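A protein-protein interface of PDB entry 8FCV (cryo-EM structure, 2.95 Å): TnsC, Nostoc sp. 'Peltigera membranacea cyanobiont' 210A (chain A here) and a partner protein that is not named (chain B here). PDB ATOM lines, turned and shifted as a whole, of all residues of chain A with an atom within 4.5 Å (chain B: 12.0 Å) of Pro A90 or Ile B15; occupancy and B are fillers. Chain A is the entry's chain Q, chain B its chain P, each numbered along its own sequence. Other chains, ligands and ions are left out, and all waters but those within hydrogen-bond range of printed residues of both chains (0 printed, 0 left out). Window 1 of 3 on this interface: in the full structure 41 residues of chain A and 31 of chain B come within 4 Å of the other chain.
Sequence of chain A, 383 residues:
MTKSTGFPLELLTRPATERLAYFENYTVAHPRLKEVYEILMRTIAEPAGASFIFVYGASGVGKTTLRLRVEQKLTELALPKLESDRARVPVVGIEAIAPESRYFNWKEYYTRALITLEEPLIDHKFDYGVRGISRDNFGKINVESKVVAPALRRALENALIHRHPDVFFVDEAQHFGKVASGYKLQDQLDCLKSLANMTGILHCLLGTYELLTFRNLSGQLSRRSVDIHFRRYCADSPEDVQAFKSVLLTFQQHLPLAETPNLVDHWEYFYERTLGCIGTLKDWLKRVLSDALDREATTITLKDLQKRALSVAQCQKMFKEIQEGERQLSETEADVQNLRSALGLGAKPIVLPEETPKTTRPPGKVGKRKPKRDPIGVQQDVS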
ATOM      1  N   THR A  75       6.849  -2.987  10.610  1.00  0.00           N
ATOM      2  CA  THR A  75       7.446  -1.667  10.768  1.00  0.00           C
ATOM      3  C   THR A  75       6.376  -0.605  10.973  1.00  0.00           C
ATOM      4  O   THR A  75       6.482   0.235  11.873  1.00  0.00           O
ATOM      5  CB  THR A  75       8.302  -1.338   9.546  1.00  0.00           C
ATOM      6  OG1 THR A  75       9.155  -2.449   9.246  1.00  0.00           O
ATOM      7  CG2 THR A  75       9.150  -0.113   9.808  1.00  0.00           C
ATOM      8  N   ALA A  78       4.702  -0.945  14.407  1.00  0.00           N
ATOM      9  CA  ALA A  78       5.513  -0.386  15.480  1.00  0.00           C
ATOM     10  C   ALA A  78       5.704   1.124  15.363  1.00  0.00           C
ATOM     11  O   ALA A  78       5.994   1.771  16.374  1.00  0.00           O
ATOM     12  CB  ALA A  78       6.876  -1.076  15.511  1.00  0.00           C
ATOM     13  N   LEU A  79       5.519   1.693  14.172  1.00  0.00           N
ATOM     14  CA  LEU A  79       5.840   3.102  13.938  1.00  0.00           C
ATOM     15  C   LEU A  79       5.231   4.077  14.939  1.00  0.00           C
ATOM     16  O   LEU A  79       5.931   5.028  15.324  1.00  0.00           O
ATOM     17  CB  LEU A  79       5.429   3.485  12.507  1.00  0.00           C
ATOM     18  CG  LEU A  79       5.748   4.916  12.073  1.00  0.00           C
ATOM     19  CD1 LEU A  79       7.245   5.078  11.832  1.00  0.00           C
ATOM     20  CD2 LEU A  79       4.959   5.306  10.834  1.00  0.00           C
ATOM     21  N   LEU A  82       7.893   4.426  17.875  1.00  0.00           N
ATOM     22  CA  LEU A  82       9.331   4.660  17.715  1.00  0.00           C
ATOM     23  C   LEU A  82       9.742   6.100  18.015  1.00  0.00           C
ATOM     24  O   LEU A  82      10.907   6.334  18.357  1.00  0.00           O
ATOM     25  CB  LEU A  82       9.805   4.271  16.307  1.00  0.00           C
ATOM     26  CG  LEU A  82      10.187   2.815  16.025  1.00  0.00           C
ATOM     27  CD1 LEU A  82      11.369   2.495  16.905  1.00  0.00           C
ATOM     28  CD2 LEU A  82       9.056   1.835  16.263  1.00  0.00           C
ATOM     29  N   ARG A  88      15.398   1.136  18.837  1.00  0.00           N
ATOM     30  CA  ARG A  88      14.297   0.181  18.914  1.00  0.00           C
ATOM     31  C   ARG A  88      13.922  -0.307  17.515  1.00  0.00           C
ATOM     32  O   ARG A  88      12.764  -0.260  17.096  1.00  0.00           O
ATOM     33  CB  ARG A  88      13.124   0.827  19.660  1.00  0.00           C
ATOM     34  CG  ARG A  88      11.890  -0.049  19.861  1.00  0.00           C
ATOM     35  CD  ARG A  88      12.236  -1.382  20.502  1.00  0.00           C
ATOM     36  NE  ARG A  88      11.071  -2.255  20.600  1.00  0.00           N
ATOM     37  CZ  ARG A  88      10.467  -2.828  19.567  1.00  0.00           C
ATOM     38  NH1 ARG A  88      10.905  -2.665  18.329  1.00  0.00           N
ATOM     39  NH2 ARG A  88       9.398  -3.589  19.783  1.00  0.00           N
ATOM     40  N   VAL A  89      14.917  -0.760  16.754  1.00  0.00           N
ATOM     41  CA  VAL A  89      14.689  -1.219  15.384  1.00  0.00           C
ATOM     42  C   VAL A  89      13.607  -2.292  15.397  1.00  0.00           C
ATOM     43  O   VAL A  89      13.747  -3.307  16.096  1.00  0.00           O
ATOM     44  CB  VAL A  89      15.986  -1.736  14.741  1.00  0.00           C
ATOM     45  CG1 VAL A  89      16.808  -0.578  14.198  1.00  0.00           C
ATOM     46  CG2 VAL A  89      16.796  -2.544  15.743  1.00  0.00           C
ATOM     47  N   PRO A  90      12.506  -2.101  14.662  1.00  0.00           N
ATOM     48  CA  PRO A  90      11.367  -3.024  14.776  1.00  0.00           C
ATOM     49  C   PRO A  90      11.688  -4.435  14.314  1.00  0.00           C
ATOM     50  O   PRO A  90      11.546  -5.392  15.080  1.00  0.00           O
ATOM     51  CB  PRO A  90      10.291  -2.378  13.890  1.00  0.00           C
ATOM     52  CG  PRO A  90      10.810  -1.020  13.518  1.00  0.00           C
ATOM     53  CD  PRO A  90      12.291  -1.066  13.640  1.00  0.00           C
ATOM     54  N   VAL A  91      12.129  -4.577  13.064  1.00  0.00           N
ATOM     55  CA  VAL A  91      12.470  -5.874  12.500  1.00  0.00           C
ATOM     56  C   VAL A  91      13.799  -5.759  11.769  1.00  0.00           C
ATOM     57  O   VAL A  91      14.206  -4.682  11.329  1.00  0.00           O
ATOM     58  CB  VAL A  91      11.381  -6.415  11.546  1.00  0.00           C
ATOM     59  CG1 VAL A  91      10.028  -6.442  12.234  1.00  0.00           C
ATOM     60  CG2 VAL A  91      11.320  -5.580  10.278  1.00  0.00           C
ATOM     61  N   PRO A 165      15.080  -6.089  18.615  1.00  0.00           N
ATOM     62  CA  PRO A 165      14.288  -6.347  17.410  1.00  0.00           C
ATOM     63  C   PRO A 165      13.173  -7.344  17.686  1.00  0.00           C
ATOM     64  O   PRO A 165      13.325  -8.272  18.484  1.00  0.00           O
ATOM     65  CB  PRO A 165      15.318  -6.920  16.433  1.00  0.00           C
ATOM     66  CG  PRO A 165      16.273  -7.643  17.321  1.00  0.00           C
ATOM     67  CD  PRO A 165      16.324  -6.881  18.628  1.00  0.00           C
ATOM     68  N   ASP A 166      12.039  -7.140  17.015  1.00  0.00           N
ATOM     69  CA  ASP A 166      10.906  -8.039  17.202  1.00  0.00           C
ATOM     70  C   ASP A 166      11.177  -9.401  16.574  1.00  0.00           C
ATOM     71  O   ASP A 166      10.928 -10.442  17.191  1.00  0.00           O
ATOM     72  CB  ASP A 166       9.638  -7.416  16.618  1.00  0.00           C
ATOM     73  CG  ASP A 166       9.186  -6.189  17.386  1.00  0.00           C
ATOM     74  OD1 ASP A 166      10.001  -5.628  18.146  1.00  0.00           O
ATOM     75  OD2 ASP A 166       8.015  -5.784  17.227  1.00  0.00           O
ATOM     76  N   VAL A 167      11.685  -9.412  15.340  1.00  0.00           N
ATOM     77  CA  VAL A 167      11.997 -10.640  14.621  1.00  0.00           C
ATOM     78  C   VAL A 167      13.356 -10.492  13.951  1.00  0.00           C
ATOM     79  O   VAL A 167      13.946  -9.409  13.920  1.00  0.00           O
ATOM     80  CB  VAL A 167      10.930 -11.002  13.563  1.00  0.00           C
ATOM     81  CG1 VAL A 167       9.534 -10.876  14.138  1.00  0.00           C
ATOM     82  CG2 VAL A 167      11.081 -10.113  12.343  1.00  0.00           C
ATOM     83  N   LEU B  10       4.588  -2.412  -1.206  1.00  0.00           N
ATOM     84  CA  LEU B  10       5.765  -2.685  -0.391  1.00  0.00           C
ATOM     85  C   LEU B  10       6.684  -1.476  -0.248  1.00  0.00           C
ATOM     86  O   LEU B  10       7.910  -1.638  -0.185  1.00  0.00           O
ATOM     87  CB  LEU B  10       6.537  -3.873  -0.970  1.00  0.00           C
ATOM     88  CG  LEU B  10       5.817  -5.225  -0.984  1.00  0.00           C
ATOM     89  CD1 LEU B  10       6.817  -6.364  -1.112  1.00  0.00           C
ATOM     90  CD2 LEU B  10       4.958  -5.400   0.260  1.00  0.00           C
ATOM     91  N   ASN B  11       6.127  -0.272  -0.198  1.00  0.00           N
ATOM     92  CA  ASN B  11       6.952   0.918  -0.049  1.00  0.00           C
ATOM     93  C   ASN B  11       7.551   0.969   1.355  1.00  0.00           C
ATOM     94  O   ASN B  11       6.933   0.488   2.313  1.00  0.00           O
ATOM     95  CB  ASN B  11       6.125   2.178  -0.312  1.00  0.00           C
ATOM     96  CG  ASN B  11       4.697   2.047   0.171  1.00  0.00           C
ATOM     97  OD1 ASN B  11       3.954   1.174  -0.277  1.00  0.00           O
ATOM     98  ND2 ASN B  11       4.301   2.918   1.092  1.00  0.00           N
ATOM     99  N   PRO B  12       8.743   1.537   1.516  1.00  0.00           N
ATOM    100  CA  PRO B  12       9.319   1.676   2.858  1.00  0.00           C
ATOM    101  C   PRO B  12       8.544   2.683   3.694  1.00  0.00           C
ATOM    102  O   PRO B  12       7.815   3.536   3.182  1.00  0.00           O
ATOM    103  CB  PRO B  12      10.747   2.160   2.586  1.00  0.00           C
ATOM    104  CG  PRO B  12      10.680   2.802   1.240  1.00  0.00           C
ATOM    105  CD  PRO B  12       9.651   2.029   0.466  1.00  0.00           C
ATOM    106  N   LEU B  13       8.718   2.574   5.014  1.00  0.00           N
ATOM    107  CA  LEU B  13       7.959   3.379   5.959  1.00  0.00           C
ATOM    108  C   LEU B  13       8.717   4.575   6.514  1.00  0.00           C
ATOM    109  O   LEU B  13       8.079   5.495   7.036  1.00  0.00           O
ATOM    110  CB  LEU B  13       7.477   2.512   7.131  1.00  0.00           C
ATOM    111  CG  LEU B  13       6.020   2.051   7.071  1.00  0.00           C
ATOM    112  CD1 LEU B  13       5.079   3.224   7.297  1.00  0.00           C
ATOM    113  CD2 LEU B  13       5.718   1.365   5.747  1.00  0.00           C
ATOM    114  N   GLU B  14      10.047   4.589   6.416  1.00  0.00           N
ATOM    115  CA  GLU B  14      10.877   5.719   6.841  1.00  0.00           C
ATOM    116  C   GLU B  14      10.652   6.023   8.330  1.00  0.00           C
ATOM    117  O   GLU B  14      10.060   7.029   8.724  1.00  0.00           O
ATOM    118  CB  GLU B  14      10.620   6.942   5.943  1.00  0.00           C
ATOM    119  CG  GLU B  14      11.255   8.291   6.354  1.00  0.00           C
ATOM    120  CD  GLU B  14      12.639   8.188   6.991  1.00  0.00           C
ATOM    121  OE1 GLU B  14      13.406   7.255   6.671  1.00  0.00           O
ATOM    122  OE2 GLU B  14      12.960   9.056   7.829  1.00  0.00           O
ATOM    123  N   ILE B  15      11.106   5.081   9.150  1.00  0.00           N
ATOM    124  CA  ILE B  15      11.075   5.234  10.604  1.00  0.00           C
ATOM    125  C   ILE B  15      12.021   6.360  11.004  1.00  0.00           C
ATOM    126  O   ILE B  15      12.965   6.666  10.261  1.00  0.00           O
ATOM    127  CB  ILE B  15      11.447   3.922  11.313  1.00  0.00           C
ATOM    128  CG1 ILE B  15      12.760   3.363  10.757  1.00  0.00           C
ATOM    129  CG2 ILE B  15      10.321   2.916  11.191  1.00  0.00           C
ATOM    130  CD1 ILE B  15      13.169   2.043  11.374  1.00  0.00           C
ATOM    131  N   PRO B  16      11.812   7.007  12.153  1.00  0.00           N
ATOM    132  CA  PRO B  16      12.725   8.076  12.574  1.00  0.00           C
ATOM    133  C   PRO B  16      14.136   7.553  12.799  1.00  0.00           C
ATOM    134  O   PRO B  16      14.356   6.375  13.090  1.00  0.00           O
ATOM    135  CB  PRO B  16      12.104   8.585  13.882  1.00  0.00           C
ATOM    136  CG  PRO B  16      11.183   7.495  14.331  1.00  0.00           C
ATOM    137  CD  PRO B  16      10.678   6.855  13.078  1.00  0.00           C
ATOM    138  N   GLN B  17      15.101   8.458  12.641  1.00  0.00           N
ATOM    139  CA  GLN B  17      16.510   8.095  12.726  1.00  0.00           C
ATOM    140  C   GLN B  17      16.832   7.456  14.070  1.00  0.00           C
ATOM    141  O   GLN B  17      16.405   7.933  15.126  1.00  0.00           O
ATOM    142  CB  GLN B  17      17.380   9.334  12.504  1.00  0.00           C
ATOM    143  CG  GLN B  17      18.865   9.049  12.357  1.00  0.00           C
ATOM    144  CD  GLN B  17      19.656   9.432  13.593  1.00  0.00           C
ATOM    145  OE1 GLN B  17      19.086   9.766  14.631  1.00  0.00           O
ATOM    146  NE2 GLN B  17      20.980   9.388  13.487  1.00  0.00           N
ATOM    147  N   ARG B  18      17.594   6.369  14.025  1.00  0.00           N
ATOM    148  CA  ARG B  18      17.949   5.607  15.212  1.00  0.00           C
ATOM    149  C   ARG B  18      19.201   6.183  15.868  1.00  0.00           C
ATOM    150  O   ARG B  18      19.965   6.935  15.258  1.00  0.00           O
ATOM    151  CB  ARG B  18      18.178   4.133  14.865  1.00  0.00           C
ATOM    152  CG  ARG B  18      17.349   3.608  13.697  1.00  0.00           C
ATOM    153  CD  ARG B  18      15.855   3.666  13.976  1.00  0.00           C
ATOM    154  NE  ARG B  18      15.541   3.357  15.367  1.00  0.00           N
ATOM    155  CZ  ARG B  18      14.579   3.945  16.065  1.00  0.00           C
ATOM    156  NH1 ARG B  18      13.813   4.881  15.531  1.00  0.00           N
ATOM    157  NH2 ARG B  18      14.383   3.584  17.329  1.00  0.00           N
ATOM    158  N   SER B  19      19.402   5.815  17.131  1.00  0.00           N
ATOM    159  CA  SER B  19      20.560   6.287  17.873  1.00  0.00           C
ATOM    160  C   SER B  19      21.843   5.669  17.326  1.00  0.00           C
ATOM    161  O   SER B  19      21.891   4.486  16.976  1.00  0.00           O
ATOM    162  CB  SER B  19      20.418   5.958  19.357  1.00  0.00           C
ATOM    163  OG  SER B  19      20.450   4.560  19.577  1.00  0.00           O
ATOM    164  N   MET B 110      20.360  10.485  21.881  1.00  0.00           N
ATOM    165  CA  MET B 110      19.151  11.266  22.170  1.00  0.00           C
ATOM    166  C   MET B 110      18.504  10.839  23.489  1.00  0.00           C
ATOM    167  O   MET B 110      17.305  10.563  23.578  1.00  0.00           O
ATOM    168  CB  MET B 110      18.149  11.253  21.000  1.00  0.00           C
ATOM    169  CG  MET B 110      17.862   9.967  20.210  1.00  0.00           C
ATOM    170  SD  MET B 110      19.289   9.222  19.401  1.00  0.00           S
ATOM    171  CE  MET B 110      19.767  10.546  18.299  1.00  0.00           C
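NH2 of Arg B18 sits close to N of Arg A88 (3.0 Å).
The backbone carbonyl oxygen (O) of Pro B16 sits at hydrogen-bond distance from the guanidinium group (NH1) of Arg B18, 2.9 Å away. NH2 of Arg A88 lies within salt-bridge range of OD1 of Asp A166, at 2.7 Å. The backbone carbonyl oxygen of Pro A90 is in hydrogen-bond range of the backbone NH of Asp A166, 2.7 Å away.
Thr A75 touches Ile B15 (CG2 to CG2, 3.5 Å). Ile B15 touches Leu A79 (CG2 to CD1, 3.8 Å). Arg B18 touches Leu A82. CD1 of Ile B15 touches CD of Pro A90, at 3.9 Å.
Of chain B, only Ile B15 comes within 4 Å of Thr A75. No residue of chain B comes within 4 Å of Ala A78. Leu A79 touches one residue of chain B. Printed residues of chain B within 4 Å of Leu A82: Arg B18. Arg A88 touches one residue of chain B. Pro A90 touches one residue of chain B. No residue of chain B comes within 4 Å of Val A91. Ile B15 touches three residues of chain A. Of the printed residues of chain A, Arg B18 touches Leu A82 (3.2 Å) and Arg A88 (3.0 Å). Ser B19 touches none of the printed residues of chain A. The nearest residue of chain B that does not touch Pro A90 is Arg B18 (5.8 Å). The nearest printed residue of chain A that does not touch Ile B15 is Leu A82 (4.8 Å).
Hydrophobic or aromatic side chains of chain A that line the printed part of chain B: Leu A79, Leu A82 and Pro A90. Along chain A the printed residues that touch a printed residue of chain B span positions 75 to 90. Hydrophobic or aromatic side chains of chain B within 4 Å of the printed part of chain A: Ile B15. Along chain B the printed residues that touch a printed residue of chain A span positions 15 to 18.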
